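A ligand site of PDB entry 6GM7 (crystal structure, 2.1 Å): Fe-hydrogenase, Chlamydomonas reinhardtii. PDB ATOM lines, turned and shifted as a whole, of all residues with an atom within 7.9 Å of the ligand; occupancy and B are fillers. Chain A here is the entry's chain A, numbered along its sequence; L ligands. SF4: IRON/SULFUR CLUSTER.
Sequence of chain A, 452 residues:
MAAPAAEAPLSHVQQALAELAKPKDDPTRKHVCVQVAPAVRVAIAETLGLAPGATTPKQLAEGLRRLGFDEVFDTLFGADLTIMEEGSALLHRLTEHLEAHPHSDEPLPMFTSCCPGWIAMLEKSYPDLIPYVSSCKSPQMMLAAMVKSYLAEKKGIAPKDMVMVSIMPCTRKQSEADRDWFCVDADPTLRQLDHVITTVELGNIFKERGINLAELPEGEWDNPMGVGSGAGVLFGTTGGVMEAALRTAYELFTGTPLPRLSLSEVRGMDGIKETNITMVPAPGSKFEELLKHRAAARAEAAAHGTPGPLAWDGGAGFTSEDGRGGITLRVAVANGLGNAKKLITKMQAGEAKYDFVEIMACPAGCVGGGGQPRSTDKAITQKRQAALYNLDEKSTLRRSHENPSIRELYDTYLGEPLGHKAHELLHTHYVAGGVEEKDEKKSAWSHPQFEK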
ATOM      1  N   ALA A  39      -4.321  32.013 -25.064  1.00  0.00           N
ATOM      2  CA  ALA A  39      -5.419  31.989 -24.109  1.00  0.00           C
ATOM      3  C   ALA A  39      -4.981  32.541 -22.753  1.00  0.00           C
ATOM      4  O   ALA A  39      -5.774  33.159 -22.042  1.00  0.00           O
ATOM      5  CB  ALA A  39      -5.946  30.570 -23.952  1.00  0.00           C
ATOM      6  N   CYS A 114      -4.322  17.899 -30.391  1.00  0.00           N
ATOM      7  CA  CYS A 114      -3.691  18.893 -29.515  1.00  0.00           C
ATOM      8  C   CYS A 114      -4.303  18.906 -28.123  1.00  0.00           C
ATOM      9  O   CYS A 114      -3.667  19.359 -27.175  1.00  0.00           O
ATOM     10  CB  CYS A 114      -3.767  20.280 -30.148  1.00  0.00           C
ATOM     11  SG  CYS A 114      -5.389  20.759 -30.733  1.00  0.00           S
ATOM     12  N   CYS A 115      -5.533  18.403 -27.985  1.00  0.00           N
ATOM     13  CA  CYS A 115      -6.181  18.358 -26.678  1.00  0.00           C
ATOM     14  C   CYS A 115      -5.906  17.036 -25.954  1.00  0.00           C
ATOM     15  O   CYS A 115      -6.391  15.985 -26.365  1.00  0.00           O
ATOM     16  CB  CYS A 115      -7.694  18.552 -26.808  1.00  0.00           C
ATOM     17  SG  CYS A 115      -8.552  18.538 -25.219  1.00  0.00           S
ATOM     18  N   PRO A 116      -5.112  17.091 -24.870  1.00  0.00           N
ATOM     19  CA  PRO A 116      -4.754  15.909 -24.074  1.00  0.00           C
ATOM     20  C   PRO A 116      -5.969  15.224 -23.458  1.00  0.00           C
ATOM     21  O   PRO A 116      -5.934  14.029 -23.217  1.00  0.00           O
ATOM     22  CB  PRO A 116      -3.833  16.476 -22.992  1.00  0.00           C
ATOM     23  CG  PRO A 116      -4.164  17.928 -22.922  1.00  0.00           C
ATOM     24  CD  PRO A 116      -4.483  18.316 -24.331  1.00  0.00           C
ATOM     25  N   GLY A 117      -7.030  15.996 -23.222  1.00  0.00           N
ATOM     26  CA  GLY A 117      -8.276  15.442 -22.727  1.00  0.00           C
ATOM     27  C   GLY A 117      -8.877  14.487 -23.744  1.00  0.00           C
ATOM     28  O   GLY A 117      -9.430  13.441 -23.378  1.00  0.00           O
ATOM     29  N   TRP A 118      -8.783  14.857 -25.017  1.00  0.00           N
ATOM     30  CA  TRP A 118      -9.251  13.998 -26.096  1.00  0.00           C
ATOM     31  C   TRP A 118      -8.345  12.777 -26.231  1.00  0.00           C
ATOM     32  O   TRP A 118      -8.825  11.654 -26.344  1.00  0.00           O
ATOM     33  CB  TRP A 118      -9.307  14.780 -27.411  1.00  0.00           C
ATOM     34  CG  TRP A 118      -9.172  13.945 -28.663  1.00  0.00           C
ATOM     35  CD1 TRP A 118      -8.267  14.123 -29.685  1.00  0.00           C
ATOM     36  CD2 TRP A 118      -9.959  12.804 -29.029  1.00  0.00           C
ATOM     37  NE1 TRP A 118      -8.453  13.175 -30.648  1.00  0.00           N
ATOM     38  CE2 TRP A 118      -9.487  12.347 -30.282  1.00  0.00           C
ATOM     39  CE3 TRP A 118     -11.022  12.121 -28.434  1.00  0.00           C
ATOM     40  CZ2 TRP A 118     -10.028  11.242 -30.935  1.00  0.00           C
ATOM     41  CZ3 TRP A 118     -11.567  11.024 -29.076  1.00  0.00           C
ATOM     42  CH2 TRP A 118     -11.072  10.601 -30.311  1.00  0.00           C
ATOM     43  N   SER A 138       1.439  18.400 -29.778  1.00  0.00           N
ATOM     44  CA  SER A 138       0.818  19.701 -29.547  1.00  0.00           C
ATOM     45  C   SER A 138       1.778  20.840 -29.893  1.00  0.00           C
ATOM     46  O   SER A 138       2.990  20.625 -29.984  1.00  0.00           O
ATOM     47  CB  SER A 138       0.387  19.825 -28.087  1.00  0.00           C
ATOM     48  OG  SER A 138       1.518  19.852 -27.240  1.00  0.00           O
ATOM     49  N   MET A 168      -0.032  27.700 -19.546  1.00  0.00           N
ATOM     50  CA  MET A 168      -1.173  27.179 -20.278  1.00  0.00           C
ATOM     51  C   MET A 168      -2.503  27.532 -19.611  1.00  0.00           C
ATOM     52  O   MET A 168      -2.538  27.780 -18.407  1.00  0.00           O
ATOM     53  CB  MET A 168      -1.044  25.657 -20.426  1.00  0.00           C
ATOM     54  CG  MET A 168       0.064  25.223 -21.380  1.00  0.00           C
ATOM     55  SD  MET A 168      -0.392  25.482 -23.115  1.00  0.00           S
ATOM     56  CE  MET A 168       1.137  26.137 -23.771  1.00  0.00           C
ATOM     57  N   PRO A 169      -3.596  27.554 -20.384  1.00  0.00           N
ATOM     58  CA  PRO A 169      -4.924  27.757 -19.812  1.00  0.00           C
ATOM     59  C   PRO A 169      -5.507  26.445 -19.331  1.00  0.00           C
ATOM     60  O   PRO A 169      -6.658  26.370 -18.896  1.00  0.00           O
ATOM     61  CB  PRO A 169      -5.732  28.311 -20.988  1.00  0.00           C
ATOM     62  CG  PRO A 169      -5.152  27.575 -22.149  1.00  0.00           C
ATOM     63  CD  PRO A 169      -3.662  27.445 -21.856  1.00  0.00           C
ATOM     64  N   CYS A 170      -4.687  25.398 -19.405  1.00  0.00           N
ATOM     65  CA  CYS A 170      -5.165  24.032 -19.312  1.00  0.00           C
ATOM     66  C   CYS A 170      -4.571  23.284 -18.121  1.00  0.00           C
ATOM     67  O   CYS A 170      -3.374  23.408 -17.836  1.00  0.00           O
ATOM     68  CB  CYS A 170      -4.853  23.291 -20.611  1.00  0.00           C
ATOM     69  SG  CYS A 170      -5.352  21.574 -20.655  1.00  0.00           S
ATOM     70  N   THR A 171      -5.396  22.503 -17.444  1.00  0.00           N
ATOM     71  CA  THR A 171      -4.952  21.724 -16.283  1.00  0.00           C
ATOM     72  C   THR A 171      -4.443  20.343 -16.705  1.00  0.00           C
ATOM     73  O   THR A 171      -4.021  19.552 -15.863  1.00  0.00           O
ATOM     74  CB  THR A 171      -6.082  21.558 -15.246  1.00  0.00           C
ATOM     75  OG1 THR A 171      -7.226  20.946 -15.862  1.00  0.00           O
ATOM     76  CG2 THR A 171      -6.489  22.918 -14.676  1.00  0.00           C
ATOM     77  N   ARG A 172      -4.485  20.054 -18.001  1.00  0.00           N
ATOM     78  CA  ARG A 172      -4.103  18.738 -18.502  1.00  0.00           C
ATOM     79  C   ARG A 172      -2.776  18.744 -19.265  1.00  0.00           C
ATOM     80  O   ARG A 172      -2.285  17.689 -19.660  1.00  0.00           O
ATOM     81  CB  ARG A 172      -5.190  18.174 -19.415  1.00  0.00           C
ATOM     82  CG  ARG A 172      -6.566  18.032 -18.772  1.00  0.00           C
ATOM     83  CD  ARG A 172      -7.496  17.324 -19.738  1.00  0.00           C
ATOM     84  NE  ARG A 172      -8.900  17.618 -19.480  1.00  0.00           N
ATOM     85  CZ  ARG A 172      -9.803  16.713 -19.134  1.00  0.00           C
ATOM     86  NH1 ARG A 172      -9.458  15.442 -19.000  1.00  0.00           N
ATOM     87  NH2 ARG A 172     -11.067  17.077 -18.926  1.00  0.00           N
ATOM     88  N   LYS A 173      -2.205  19.929 -19.475  1.00  0.00           N
ATOM     89  CA  LYS A 173      -0.998  20.060 -20.297  1.00  0.00           C
ATOM     90  C   LYS A 173       0.253  19.523 -19.610  1.00  0.00           C
ATOM     91  O   LYS A 173       1.265  19.276 -20.260  1.00  0.00           O
ATOM     92  CB  LYS A 173      -0.803  21.522 -20.706  1.00  0.00           C
ATOM     93  CG  LYS A 173      -1.691  21.958 -21.860  1.00  0.00           C
ATOM     94  CD  LYS A 173      -1.387  21.152 -23.112  1.00  0.00           C
ATOM     95  CE  LYS A 173      -2.348  21.463 -24.245  1.00  0.00           C
ATOM     96  NZ  LYS A 173      -1.994  20.719 -25.485  1.00  0.00           N
ATOM     97  N   GLU A 176       0.171  15.812 -20.500  1.00  0.00           N
ATOM     98  CA  GLU A 176       0.628  15.724 -21.879  1.00  0.00           C
ATOM     99  C   GLU A 176       2.147  15.755 -21.924  1.00  0.00           C
ATOM    100  O   GLU A 176       2.775  14.924 -22.582  1.00  0.00           O
ATOM    101  CB  GLU A 176       0.043  16.859 -22.724  1.00  0.00           C
ATOM    102  CG  GLU A 176       0.588  16.916 -24.144  1.00  0.00           C
ATOM    103  CD  GLU A 176       0.146  18.171 -24.884  1.00  0.00           C
ATOM    104  OE1 GLU A 176      -1.012  18.199 -25.377  1.00  0.00           O
ATOM    105  OE2 GLU A 176       0.943  19.119 -24.972  1.00  0.00           O
ATOM    106  N   ALA A 334     -15.948  19.370 -32.156  1.00  0.00           N
ATOM    107  CA  ALA A 334     -16.712  18.936 -30.996  1.00  0.00           C
ATOM    108  C   ALA A 334     -16.193  19.539 -29.683  1.00  0.00           C
ATOM    109  O   ALA A 334     -15.031  19.376 -29.332  1.00  0.00           O
ATOM    110  CB  ALA A 334     -16.700  17.418 -30.896  1.00  0.00           C
ATOM    111  N   ASN A 335     -17.086  20.233 -28.987  1.00  0.00           N
ATOM    112  CA  ASN A 335     -16.865  20.704 -27.623  1.00  0.00           C
ATOM    113  C   ASN A 335     -18.059  20.295 -26.746  1.00  0.00           C
ATOM    114  O   ASN A 335     -19.176  20.717 -27.018  1.00  0.00           O
ATOM    115  CB  ASN A 335     -16.701  22.236 -27.580  1.00  0.00           C
ATOM    116  CG  ASN A 335     -15.591  22.756 -28.485  1.00  0.00           C
ATOM    117  OD1 ASN A 335     -14.473  23.005 -28.035  1.00  0.00           O
ATOM    118  ND2 ASN A 335     -15.904  22.956 -29.763  1.00  0.00           N
ATOM    119  N   GLY A 336     -17.852  19.479 -25.709  1.00  0.00           N
ATOM    120  CA  GLY A 336     -16.573  18.895 -25.356  1.00  0.00           C
ATOM    121  C   GLY A 336     -16.651  17.379 -25.339  1.00  0.00           C
ATOM    122  O   GLY A 336     -17.184  16.779 -26.272  1.00  0.00           O
ATOM    123  N   LEU A 337     -16.148  16.747 -24.284  1.00  0.00           N
ATOM    124  CA  LEU A 337     -15.963  15.301 -24.282  1.00  0.00           C
ATOM    125  C   LEU A 337     -17.273  14.515 -24.268  1.00  0.00           C
ATOM    126  O   LEU A 337     -17.351  13.439 -24.880  1.00  0.00           O
ATOM    127  CB  LEU A 337     -15.097  14.876 -23.088  1.00  0.00           C
ATOM    128  CG  LEU A 337     -13.632  15.299 -23.168  1.00  0.00           C
ATOM    129  CD1 LEU A 337     -12.815  14.696 -22.043  1.00  0.00           C
ATOM    130  CD2 LEU A 337     -13.034  14.911 -24.520  1.00  0.00           C
ATOM    131  N   ILE A 359     -11.560  17.481 -31.735  1.00  0.00           N
ATOM    132  CA  ILE A 359     -12.206  17.311 -30.451  1.00  0.00           C
ATOM    133  C   ILE A 359     -11.490  18.086 -29.352  1.00  0.00           C
ATOM    134  O   ILE A 359     -10.311  17.843 -29.071  1.00  0.00           O
ATOM    135  CB  ILE A 359     -12.288  15.826 -30.064  1.00  0.00           C
ATOM    136  CG1 ILE A 359     -13.179  15.075 -31.049  1.00  0.00           C
ATOM    137  CG2 ILE A 359     -12.788  15.668 -28.634  1.00  0.00           C
ATOM    138  CD1 ILE A 359     -13.183  13.566 -30.878  1.00  0.00           C
ATOM    139  N   MET A 360     -12.197  19.039 -28.747  1.00  0.00           N
ATOM    140  CA  MET A 360     -11.690  19.790 -27.599  1.00  0.00           C
ATOM    141  C   MET A 360     -12.485  19.407 -26.367  1.00  0.00           C
ATOM    142  O   MET A 360     -13.709  19.337 -26.408  1.00  0.00           O
ATOM    143  CB  MET A 360     -11.791  21.296 -27.835  1.00  0.00           C
ATOM    144  CG  MET A 360     -10.975  21.841 -28.994  1.00  0.00           C
ATOM    145  SD  MET A 360      -9.200  21.858 -28.639  1.00  0.00           S
ATOM    146  CE  MET A 360      -8.669  20.580 -29.760  1.00  0.00           C
ATOM    147  N   ALA A 361     -11.809  19.171 -25.248  1.00  0.00           N
ATOM    148  CA  ALA A 361     -12.476  18.762 -24.022  1.00  0.00           C
ATOM    149  C   ALA A 361     -13.309  19.891 -23.418  1.00  0.00           C
ATOM    150  O   ALA A 361     -14.367  19.653 -22.827  1.00  0.00           O
ATOM    151  CB  ALA A 361     -11.468  18.251 -23.005  1.00  0.00           C
ATOM    152  N   CYS A 362     -12.842  21.127 -23.561  1.00  0.00           N
ATOM    153  CA  CYS A 362     -13.541  22.271 -22.983  1.00  0.00           C
ATOM    154  C   CYS A 362     -14.648  22.781 -23.892  1.00  0.00           C
ATOM    155  O   CYS A 362     -14.453  22.918 -25.100  1.00  0.00           O
ATOM    156  CB  CYS A 362     -12.554  23.394 -22.655  1.00  0.00           C
ATOM    157  SG  CYS A 362     -11.359  22.951 -21.377  1.00  0.00           S
ATOM    158  N   PRO A 363     -15.828  23.062 -23.309  1.00  0.00           N
ATOM    159  CA  PRO A 363     -16.991  23.586 -24.042  1.00  0.00           C
ATOM    160  C   PRO A 363     -16.691  24.850 -24.845  1.00  0.00           C
ATOM    161  O   PRO A 363     -17.175  24.964 -25.970  1.00  0.00           O
ATOM    162  CB  PRO A 363     -17.984  23.888 -22.915  1.00  0.00           C
ATOM    163  CG  PRO A 363     -17.650  22.906 -21.858  1.00  0.00           C
ATOM    164  CD  PRO A 363     -16.143  22.779 -21.903  1.00  0.00           C
ATOM    165  N   ALA A 364     -15.918  25.766 -24.291  1.00  0.00           N
ATOM    166  CA  ALA A 364     -15.613  27.019 -24.973  1.00  0.00           C
ATOM    167  C   ALA A 364     -14.212  26.989 -25.585  1.00  0.00           C
ATOM    168  O   ALA A 364     -13.707  28.020 -26.027  1.00  0.00           O
ATOM    169  CB  ALA A 364     -15.742  28.185 -24.014  1.00  0.00           C
ATOM    170  N   GLY A 365     -13.601  25.816 -25.614  1.00  0.00           N
ATOM    171  CA  GLY A 365     -12.239  25.699 -26.105  1.00  0.00           C
ATOM    172  C   GLY A 365     -11.234  26.174 -25.064  1.00  0.00           C
ATOM    173  O   GLY A 365     -11.582  26.390 -23.909  1.00  0.00           O
ATOM    174  N   CYS A 366      -9.991  26.372 -25.495  1.00  0.00           N
ATOM    175  CA  CYS A 366      -8.906  26.651 -24.563  1.00  0.00           C
ATOM    176  C   CYS A 366      -9.082  27.965 -23.797  1.00  0.00           C
ATOM    177  O   CYS A 366      -8.551  28.108 -22.694  1.00  0.00           O
ATOM    178  CB  CYS A 366      -7.571  26.660 -25.308  1.00  0.00           C
ATOM    179  SG  CYS A 366      -7.048  25.029 -25.889  1.00  0.00           S
ATOM    180  N   VAL A 367      -9.828  28.905 -24.363  1.00  0.00           N
ATOM    181  CA  VAL A 367     -10.060  30.181 -23.677  1.00  0.00           C
ATOM    182  C   VAL A 367     -10.904  29.976 -22.424  1.00  0.00           C
ATOM    183  O   VAL A 367     -10.917  30.826 -21.534  1.00  0.00           O
ATOM    184  CB  VAL A 367     -10.744  31.219 -24.595  1.00  0.00           C
ATOM    185  CG1 VAL A 367      -9.774  31.711 -25.667  1.00  0.00           C
ATOM    186  CG2 VAL A 367     -12.007  30.632 -25.221  1.00  0.00           C
ATOM    187  N   GLY A 368     -11.621  28.857 -22.372  1.00  0.00           N
ATOM    188  CA  GLY A 368     -12.395  28.496 -21.197  1.00  0.00           C
ATOM    189  C   GLY A 368     -11.841  27.256 -20.518  1.00  0.00           C
ATOM    190  O   GLY A 368     -12.600  26.447 -19.975  1.00  0.00           O
ATOM    191  N   GLY A 369     -10.523  27.107 -20.556  1.00  0.00           N
ATOM    192  CA  GLY A 369      -9.856  25.958 -19.952  1.00  0.00           C
ATOM    193  C   GLY A 369      -9.910  25.962 -18.444  1.00  0.00           C
ATOM    194  O   GLY A 369     -10.254  26.962 -17.815  1.00  0.00           O
ATOM    195  N   GLY A 370      -9.550  24.821 -17.854  1.00  0.00           N
ATOM    196  CA  GLY A 370      -9.635  24.634 -16.409  1.00  0.00           C
ATOM    197  C   GLY A 370      -8.643  25.448 -15.599  1.00  0.00           C
ATOM    198  O   GLY A 370      -8.792  25.594 -14.395  1.00  0.00           O
ATOM    199  N   GLY A 371      -7.619  25.980 -16.271  1.00  0.00           N
ATOM    200  CA  GLY A 371      -6.601  26.768 -15.600  1.00  0.00           C
ATOM    201  C   GLY A 371      -6.875  28.260 -15.683  1.00  0.00           C
ATOM    202  O   GLY A 371      -6.078  29.080 -15.220  1.00  0.00           O
ATOM    203  N   GLN A 372      -8.013  28.613 -16.275  1.00  0.00           N
ATOM    204  CA  GLN A 372      -8.384  30.017 -16.466  1.00  0.00           C
ATOM    205  C   GLN A 372      -9.052  30.579 -15.215  1.00  0.00           C
ATOM    206  O   GLN A 372      -9.638  29.827 -14.425  1.00  0.00           O
ATOM    207  CB  GLN A 372      -9.305  30.156 -17.674  1.00  0.00           C
ATOM    208  CG  GLN A 372      -8.687  29.752 -18.999  1.00  0.00           C
ATOM    209  CD  GLN A 372      -7.666  30.765 -19.513  1.00  0.00           C
ATOM    210  OE1 GLN A 372      -6.627  30.974 -18.891  1.00  0.00           O
ATOM    211  NE2 GLN A 372      -7.969  31.388 -20.641  1.00  0.00           N
HETATM  212 FE1  SF4 L   1      -8.286  20.638 -24.318  1.00  0.00          FE
HETATM  213 FE2  SF4 L   1      -9.444  22.358 -22.503  1.00  0.00          FE
HETATM  214 FE3  SF4 L   1      -6.737  21.927 -22.453  1.00  0.00          FE
HETATM  215 FE4  SF4 L   1      -7.856  23.344 -24.531  1.00  0.00          FE
HETATM  216  S1  SF4 L   1      -7.807  23.954 -22.304  1.00  0.00           S
HETATM  217  S2  SF4 L   1      -6.268  21.695 -24.692  1.00  0.00           S
HETATM  218  S3  SF4 L   1      -9.866  22.236 -24.769  1.00  0.00           S
HETATM  219  S4  SF4 L   1      -8.373  20.391 -22.036  1.00  0.00           S
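The side-chain sulfur (SG) of Cys 170 binds an iron atom (FE3) of the ligand. A sulfur (S3) of the ligand lies close to the backbone NH (N) of Cys 362, at 3.4 Å. The side-chain sulfur of Cys 362 is bound to an iron atom (FE2) of the ligand, at 2.3 Å. An iron atom (FE1) of the ligand is bound by the side-chain sulfur (SG) of Cys 115 (2.3 Å). The side-chain sulfur of Cys 366 is bound to an iron atom (FE4) of the ligand (2.3 Å). The backbone NH (N) of Ala 361 lies close to a sulfur (S3) of the ligand, 3.7 Å away.
Residues that only touch the ligand: Gly 369, Met 360, Arg 172, Pro 116 and Lys 173.
N of Arg 172 sits close to SG of Cys 170 (3.2 Å). N of Lys 173 lies close to SG of Cys 170, at 3.7 Å. OD1 of Asn 335 lies close to O of Cys 362. The backbone NH (N) of Ala 361 lies close to the side-chain sulfur (SG) of Cys 115 (3.3 Å). The side-chain sulfur of Cys 115 sits close to the backbone NH of Gly 117 (3.6 Å). The backbone NH (N) of Trp 118 sits close to the side-chain sulfur (SG) of Cys 115, at 3.7 Å. The side-chain amino group (NZ) of Lys 173 lies within hydrogen-bond range of the backbone carbonyl oxygen (O) of Cys 114. The side-chain carboxylate (OE1) of Glu 176 is in salt-bridge range of the side-chain amino group (NZ) of Lys 173, 2.7 Å away.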
